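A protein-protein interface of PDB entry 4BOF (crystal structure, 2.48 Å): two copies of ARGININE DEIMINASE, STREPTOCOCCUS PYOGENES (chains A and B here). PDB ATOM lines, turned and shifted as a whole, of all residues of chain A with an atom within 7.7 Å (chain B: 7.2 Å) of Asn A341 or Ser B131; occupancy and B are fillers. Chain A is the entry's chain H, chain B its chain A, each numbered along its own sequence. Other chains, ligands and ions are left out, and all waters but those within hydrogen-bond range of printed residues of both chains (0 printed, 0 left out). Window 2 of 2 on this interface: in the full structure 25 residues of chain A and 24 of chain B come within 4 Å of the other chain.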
ATOM      1  N   PRO A 292      -9.102  21.194  16.172  1.00  0.00           N
ATOM      2  CA  PRO A 292      -8.038  21.455  15.181  1.00  0.00           C
ATOM      3  C   PRO A 292      -7.338  22.823  15.293  1.00  0.00           C
ATOM      4  O   PRO A 292      -6.111  22.859  15.215  1.00  0.00           O
ATOM      5  CB  PRO A 292      -8.766  21.324  13.836  1.00  0.00           C
ATOM      6  CG  PRO A 292     -10.221  21.452  14.159  1.00  0.00           C
ATOM      7  CD  PRO A 292     -10.374  20.843  15.508  1.00  0.00           C
ATOM      8  N   ARG A 336      -9.489  14.557  15.265  1.00  0.00           N
ATOM      9  CA  ARG A 336     -10.070  15.874  14.953  1.00  0.00           C
ATOM     10  C   ARG A 336     -11.535  15.959  15.300  1.00  0.00           C
ATOM     11  O   ARG A 336     -12.330  15.226  14.718  1.00  0.00           O
ATOM     12  CB  ARG A 336      -9.912  16.202  13.455  1.00  0.00           C
ATOM     13  CG  ARG A 336      -8.527  16.667  13.035  1.00  0.00           C
ATOM     14  CD  ARG A 336      -8.112  15.985  11.744  1.00  0.00           C
ATOM     15  NE  ARG A 336      -6.864  15.234  11.908  1.00  0.00           N
ATOM     16  CZ  ARG A 336      -6.772  14.014  12.435  1.00  0.00           C
ATOM     17  NH1 ARG A 336      -7.860  13.381  12.860  1.00  0.00           N
ATOM     18  NH2 ARG A 336      -5.591  13.418  12.543  1.00  0.00           N
ATOM     19  N   CYS A 337     -11.910  16.887  16.200  1.00  0.00           N
ATOM     20  CA  CYS A 337     -13.322  17.147  16.553  1.00  0.00           C
ATOM     21  C   CYS A 337     -13.974  17.738  15.325  1.00  0.00           C
ATOM     22  O   CYS A 337     -13.425  18.674  14.759  1.00  0.00           O
ATOM     23  CB  CYS A 337     -13.408  18.093  17.756  1.00  0.00           C
ATOM     24  SG  CYS A 337     -15.071  18.746  18.117  1.00  0.00           S
ATOM     25  N   GLY A 338     -15.067  17.155  14.867  1.00  0.00           N
ATOM     26  CA  GLY A 338     -15.808  17.639  13.697  1.00  0.00           C
ATOM     27  C   GLY A 338     -15.216  17.331  12.335  1.00  0.00           C
ATOM     28  O   GLY A 338     -15.691  17.844  11.318  1.00  0.00           O
ATOM     29  N   GLY A 339     -14.195  16.484  12.312  1.00  0.00           N
ATOM     30  CA  GLY A 339     -13.510  16.073  11.088  1.00  0.00           C
ATOM     31  C   GLY A 339     -12.693  17.159  10.435  1.00  0.00           C
ATOM     32  O   GLY A 339     -12.173  18.049  11.112  1.00  0.00           O
ATOM     33  N   ASP A 340     -12.599  17.092   9.096  1.00  0.00           N
ATOM     34  CA  ASP A 340     -11.848  18.020   8.246  1.00  0.00           C
ATOM     35  C   ASP A 340     -12.634  19.303   7.895  1.00  0.00           C
ATOM     36  O   ASP A 340     -12.011  20.341   7.667  1.00  0.00           O
ATOM     37  CB  ASP A 340     -11.399  17.298   6.968  1.00  0.00           C
ATOM     38  CG  ASP A 340     -10.542  16.044   7.224  1.00  0.00           C
ATOM     39  OD1 ASP A 340      -9.651  16.092   8.122  1.00  0.00           O
ATOM     40  OD2 ASP A 340     -10.758  15.020   6.525  1.00  0.00           O
ATOM     41  N   ASN A 341     -13.978  19.241   7.888  1.00  0.00           N
ATOM     42  CA  ASN A 341     -14.884  20.363   7.613  1.00  0.00           C
ATOM     43  C   ASN A 341     -14.874  21.383   8.771  1.00  0.00           C
ATOM     44  O   ASN A 341     -15.141  21.030   9.920  1.00  0.00           O
ATOM     45  CB  ASN A 341     -16.306  19.838   7.349  1.00  0.00           C
ATOM     46  CG  ASN A 341     -17.269  20.895   6.921  1.00  0.00           C
ATOM     47  OD1 ASN A 341     -17.953  21.532   7.726  1.00  0.00           O
ATOM     48  ND2 ASN A 341     -17.349  21.101   5.636  1.00  0.00           N
ATOM     49  N   LEU A 342     -14.565  22.649   8.445  1.00  0.00           N
ATOM     50  CA  LEU A 342     -14.487  23.793   9.378  1.00  0.00           C
ATOM     51  C   LEU A 342     -15.805  24.082  10.097  1.00  0.00           C
ATOM     52  O   LEU A 342     -15.788  24.352  11.303  1.00  0.00           O
ATOM     53  CB  LEU A 342     -14.070  25.080   8.638  1.00  0.00           C
ATOM     54  CG  LEU A 342     -12.625  25.226   8.181  1.00  0.00           C
ATOM     55  CD1 LEU A 342     -12.511  26.343   7.142  1.00  0.00           C
ATOM     56  CD2 LEU A 342     -11.696  25.535   9.362  1.00  0.00           C
ATOM     57  N   VAL A 343     -16.928  24.070   9.346  1.00  0.00           N
ATOM     58  CA  VAL A 343     -18.269  24.356   9.859  1.00  0.00           C
ATOM     59  C   VAL A 343     -18.666  23.299  10.895  1.00  0.00           C
ATOM     60  O   VAL A 343     -19.071  23.671  12.004  1.00  0.00           O
ATOM     61  CB  VAL A 343     -19.331  24.498   8.732  1.00  0.00           C
ATOM     62  CG1 VAL A 343     -20.687  24.904   9.307  1.00  0.00           C
ATOM     63  CG2 VAL A 343     -18.879  25.516   7.687  1.00  0.00           C
ATOM     64  N   ALA A 344     -18.495  21.992  10.547  1.00  0.00           N
ATOM     65  CA  ALA A 344     -18.818  20.853  11.407  1.00  0.00           C
ATOM     66  C   ALA A 344     -18.012  20.901  12.693  1.00  0.00           C
ATOM     67  O   ALA A 344     -18.579  20.682  13.768  1.00  0.00           O
ATOM     68  CB  ALA A 344     -18.563  19.552  10.671  1.00  0.00           C
ATOM     69  N   ALA A 345     -16.705  21.235  12.586  1.00  0.00           N
ATOM     70  CA  ALA A 345     -15.760  21.368  13.704  1.00  0.00           C
ATOM     71  C   ALA A 345     -16.160  22.491  14.658  1.00  0.00           C
ATOM     72  O   ALA A 345     -16.120  22.276  15.859  1.00  0.00           O
ATOM     73  CB  ALA A 345     -14.335  21.593  13.192  1.00  0.00           C
ATOM     74  N   GLY A 346     -16.556  23.640  14.123  1.00  0.00           N
ATOM     75  CA  GLY A 346     -16.980  24.785  14.910  1.00  0.00           C
ATOM     76  C   GLY A 346     -18.249  24.486  15.688  1.00  0.00           C
ATOM     77  O   GLY A 346     -18.320  24.748  16.891  1.00  0.00           O
ATOM     78  N   ARG A 347     -19.229  23.871  15.011  1.00  0.00           N
ATOM     79  CA  ARG A 347     -20.531  23.493  15.537  1.00  0.00           C
ATOM     80  C   ARG A 347     -20.379  22.496  16.692  1.00  0.00           C
ATOM     81  O   ARG A 347     -20.959  22.672  17.774  1.00  0.00           O
ATOM     82  CB  ARG A 347     -21.334  22.881  14.369  1.00  0.00           C
ATOM     83  CG  ARG A 347     -22.745  22.371  14.689  1.00  0.00           C
ATOM     84  CD  ARG A 347     -23.309  21.408  13.633  1.00  0.00           C
ATOM     85  NE  ARG A 347     -22.907  21.719  12.251  1.00  0.00           N
ATOM     86  CZ  ARG A 347     -22.563  20.792  11.355  1.00  0.00           C
ATOM     87  NH1 ARG A 347     -22.606  19.504  11.670  1.00  0.00           N
ATOM     88  NH2 ARG A 347     -22.201  21.145  10.126  1.00  0.00           N
ATOM     89  N   ILE A 372     -20.707  13.932  13.774  1.00  0.00           N
ATOM     90  CA  ILE A 372     -19.441  13.801  13.038  1.00  0.00           C
ATOM     91  C   ILE A 372     -18.316  13.289  13.948  1.00  0.00           C
ATOM     92  O   ILE A 372     -17.615  12.368  13.535  1.00  0.00           O
ATOM     93  CB  ILE A 372     -19.025  15.111  12.299  1.00  0.00           C
ATOM     94  CG1 ILE A 372     -20.180  15.742  11.459  1.00  0.00           C
ATOM     95  CG2 ILE A 372     -17.734  14.943  11.470  1.00  0.00           C
ATOM     96  CD1 ILE A 372     -20.957  14.887  10.443  1.00  0.00           C
ATOM     97  N   GLU B  29     -27.593  23.516   9.997  1.00  0.00           N
ATOM     98  CA  GLU B  29     -26.297  22.826  10.087  1.00  0.00           C
ATOM     99  C   GLU B  29     -25.172  23.784   9.791  1.00  0.00           C
ATOM    100  O   GLU B  29     -24.053  23.593  10.269  1.00  0.00           O
ATOM    101  CB  GLU B  29     -26.252  21.676   9.078  1.00  0.00           C
ATOM    102  CG  GLU B  29     -26.183  20.298   9.689  1.00  0.00           C
ATOM    103  CD  GLU B  29     -25.952  19.208   8.659  1.00  0.00           C
ATOM    104  OE1 GLU B  29     -25.101  19.402   7.755  1.00  0.00           O
ATOM    105  OE2 GLU B  29     -26.627  18.156   8.754  1.00  0.00           O
ATOM    106  N   ASN B  30     -25.460  24.804   8.977  1.00  0.00           N
ATOM    107  CA  ASN B  30     -24.505  25.828   8.531  1.00  0.00           C
ATOM    108  C   ASN B  30     -24.420  27.008   9.515  1.00  0.00           C
ATOM    109  O   ASN B  30     -24.086  28.127   9.149  1.00  0.00           O
ATOM    110  CB  ASN B  30     -24.856  26.288   7.117  1.00  0.00           C
ATOM    111  CG  ASN B  30     -24.389  25.301   6.078  1.00  0.00           C
ATOM    112  OD1 ASN B  30     -23.430  24.541   6.300  1.00  0.00           O
ATOM    113  ND2 ASN B  30     -25.042  25.292   4.916  1.00  0.00           N
ATOM    114  N   VAL B 128     -24.077  28.097   0.727  1.00  0.00           N
ATOM    115  CA  VAL B 128     -22.928  27.364   0.154  1.00  0.00           C
ATOM    116  C   VAL B 128     -21.664  27.628   0.967  1.00  0.00           C
ATOM    117  O   VAL B 128     -21.289  28.796   1.159  1.00  0.00           O
ATOM    118  CB  VAL B 128     -22.697  27.749  -1.336  1.00  0.00           C
ATOM    119  CG1 VAL B 128     -21.520  27.003  -1.931  1.00  0.00           C
ATOM    120  CG2 VAL B 128     -23.929  27.524  -2.180  1.00  0.00           C
ATOM    121  N   GLN B 129     -20.996  26.547   1.417  1.00  0.00           N
ATOM    122  CA  GLN B 129     -19.675  26.651   2.082  1.00  0.00           C
ATOM    123  C   GLN B 129     -18.598  26.832   1.001  1.00  0.00           C
ATOM    124  O   GLN B 129     -18.752  26.292  -0.095  1.00  0.00           O
ATOM    125  CB  GLN B 129     -19.362  25.408   2.902  1.00  0.00           C
ATOM    126  CG  GLN B 129     -20.278  25.217   4.095  1.00  0.00           C
ATOM    127  CD  GLN B 129     -19.949  23.956   4.857  1.00  0.00           C
ATOM    128  OE1 GLN B 129     -18.815  23.475   4.832  1.00  0.00           O
ATOM    129  NE2 GLN B 129     -20.913  23.445   5.627  1.00  0.00           N
ATOM    130  N   LYS B 130     -17.510  27.570   1.307  1.00  0.00           N
ATOM    131  CA  LYS B 130     -16.413  27.796   0.370  1.00  0.00           C
ATOM    132  C   LYS B 130     -15.752  26.476  -0.005  1.00  0.00           C
ATOM    133  O   LYS B 130     -15.333  26.313  -1.166  1.00  0.00           O
ATOM    134  CB  LYS B 130     -15.375  28.777   0.936  1.00  0.00           C
ATOM    135  CG  LYS B 130     -15.820  30.229   0.897  1.00  0.00           C
ATOM    136  CD  LYS B 130     -14.763  31.122   1.531  1.00  0.00           C
ATOM    137  CE  LYS B 130     -15.227  32.551   1.630  1.00  0.00           C
ATOM    138  NZ  LYS B 130     -14.267  33.380   2.403  1.00  0.00           N
ATOM    139  N   SER B 131     -15.712  25.522   0.966  1.00  0.00           N
ATOM    140  CA  SER B 131     -15.121  24.185   0.794  1.00  0.00           C
ATOM    141  C   SER B 131     -15.811  23.373  -0.320  1.00  0.00           C
ATOM    142  O   SER B 131     -15.155  22.552  -0.948  1.00  0.00           O
ATOM    143  CB  SER B 131     -15.162  23.410   2.107  1.00  0.00           C
ATOM    144  OG  SER B 131     -16.492  23.154   2.539  1.00  0.00           O
ATOM    145  N   GLU B 132     -17.103  23.647  -0.595  1.00  0.00           N
ATOM    146  CA  GLU B 132     -17.929  22.980  -1.603  1.00  0.00           C
ATOM    147  C   GLU B 132     -17.599  23.397  -3.026  1.00  0.00           C
ATOM    148  O   GLU B 132     -18.100  22.771  -3.977  1.00  0.00           O
ATOM    149  CB  GLU B 132     -19.407  23.320  -1.372  1.00  0.00           C
ATOM    150  CG  GLU B 132     -20.011  22.844  -0.060  1.00  0.00           C
ATOM    151  CD  GLU B 132     -21.441  23.310   0.101  1.00  0.00           C
ATOM    152  OE1 GLU B 132     -22.125  23.441  -0.936  1.00  0.00           O
ATOM    153  OE2 GLU B 132     -21.874  23.551   1.249  1.00  0.00           O
ATOM    154  N   LEU B 133     -16.849  24.508  -3.182  1.00  0.00           N
ATOM    155  CA  LEU B 133     -16.531  25.082  -4.489  1.00  0.00           C
ATOM    156  C   LEU B 133     -15.142  24.684  -4.995  1.00  0.00           C
ATOM    157  O   LEU B 133     -14.178  24.664  -4.204  1.00  0.00           O
ATOM    158  CB  LEU B 133     -16.659  26.608  -4.461  1.00  0.00           C
ATOM    159  CG  LEU B 133     -18.079  27.148  -4.172  1.00  0.00           C
ATOM    160  CD1 LEU B 133     -18.083  28.651  -4.077  1.00  0.00           C
ATOM    161  CD2 LEU B 133     -19.086  26.698  -5.211  1.00  0.00           C
ATOM    162  N   PRO B 134     -15.033  24.381  -6.326  1.00  0.00           N
ATOM    163  CA  PRO B 134     -13.733  23.999  -6.897  1.00  0.00           C
ATOM    164  C   PRO B 134     -12.732  25.139  -6.851  1.00  0.00           C
ATOM    165  O   PRO B 134     -13.125  26.307  -6.723  1.00  0.00           O
ATOM    166  CB  PRO B 134     -14.082  23.626  -8.342  1.00  0.00           C
ATOM    167  CG  PRO B 134     -15.305  24.373  -8.649  1.00  0.00           C
ATOM    168  CD  PRO B 134     -16.082  24.379  -7.373  1.00  0.00           C
ATOM    169  N   PRO B 152     -16.141  31.136   6.416  1.00  0.00           N
ATOM    170  CA  PRO B 152     -16.323  29.851   5.724  1.00  0.00           C
ATOM    171  C   PRO B 152     -17.452  29.758   4.686  1.00  0.00           C
ATOM    172  O   PRO B 152     -17.473  28.771   3.956  1.00  0.00           O
ATOM    173  CB  PRO B 152     -16.585  28.888   6.874  1.00  0.00           C
ATOM    174  CG  PRO B 152     -17.257  29.723   7.894  1.00  0.00           C
ATOM    175  CD  PRO B 152     -16.703  31.096   7.778  1.00  0.00           C
ATOM    176  N   PHE B 153     -18.351  30.747   4.588  1.00  0.00           N
ATOM    177  CA  PHE B 153     -19.462  30.697   3.630  1.00  0.00           C
ATOM    178  C   PHE B 153     -19.286  31.587   2.420  1.00  0.00           C
ATOM    179  O   PHE B 153     -18.851  32.731   2.546  1.00  0.00           O
ATOM    180  CB  PHE B 153     -20.793  31.061   4.313  1.00  0.00           C
ATOM    181  CG  PHE B 153     -21.101  30.162   5.483  1.00  0.00           C
ATOM    182  CD1 PHE B 153     -21.471  28.833   5.281  1.00  0.00           C
ATOM    183  CD2 PHE B 153     -20.934  30.613   6.789  1.00  0.00           C
ATOM    184  CE1 PHE B 153     -21.675  27.978   6.365  1.00  0.00           C
ATOM    185  CE2 PHE B 153     -21.168  29.766   7.876  1.00  0.00           C
ATOM    186  CZ  PHE B 153     -21.528  28.454   7.656  1.00  0.00           C
ATOM    187  N   ALA B 154     -19.653  31.043   1.238  1.00  0.00           N
ATOM    188  CA  ALA B 154     -19.700  31.754  -0.046  1.00  0.00           C
ATOM    189  C   ALA B 154     -21.086  32.419  -0.154  1.00  0.00           C
ATOM    190  O   ALA B 154     -21.225  33.540  -0.639  1.00  0.00           O
ATOM    191  CB  ALA B 154     -19.457  30.792  -1.189  1.00  0.00           C
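Hydrophobic or aromatic side chains of chain A within 4 Å of the printed part of chain B: Val A343.
Among the printed residues, no Asp or Glu carboxylate lies within 4 Å of a Lys or Arg side-chain nitrogen of the other chain.
The side-chain amide nitrogen (NE2) of Gln B129 sits at hydrogen-bond distance from the side-chain amide oxygen (OD1) of Asn B30 (2.8 Å).
OG of Ser B131 sits at hydrogen-bond distance from OE1 of Gln B129 (3.3 Å).
The backbone NH (N) of Gln B129 sits at hydrogen-bond distance from the side-chain carboxylate (OE2) of Glu B132 (3.1 Å).
OD1 of Asn A341 sits at hydrogen-bond distance from N of Val A343 (3.2 Å).
The backbone NH (N) of Ala A344 lies within hydrogen-bond range of the side-chain amide oxygen (OD1) of Asn A341, at 2.9 Å.
No position is printed for both chains.
Of the 6 pairs that touch across the chains among the printed residues, none has its exchanged pair printed and touching as well.
OG of Ser B131 touches ND2 of Asn A341, at 3.8 Å.
O of Glu B29 touches CG1 of Val A343 (3.7 Å).
CG2 of Val A343 touches CD of Gln B129, at 3.4 Å.
Val A343 touches Phe B153.
Asn A341 touches two residues of chain B.
Of the printed residues of chain A, Glu B29 touches Val A343 and Arg A347.
Of the printed residues of chain B, Arg A347 touches Glu B29.
Ile A372 touches none of the printed residues of chain B.
Gly A338 touches none of the printed residues of chain B.
The nearest residue of chain B that does not touch Asn A341 is Asn B30 (6.4 Å).
The nearest printed residue of chain A that does not touch Gln B129 is Arg A347 (5.2 Å).
The guanidinium group of Arg A347 sits at hydrogen-bond distance from the backbone carbonyl oxygen of Glu B29 (3.0 Å).
The side-chain amide oxygen of Gln B129 is in hydrogen-bond range of the side-chain amide nitrogen of Asn A341.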
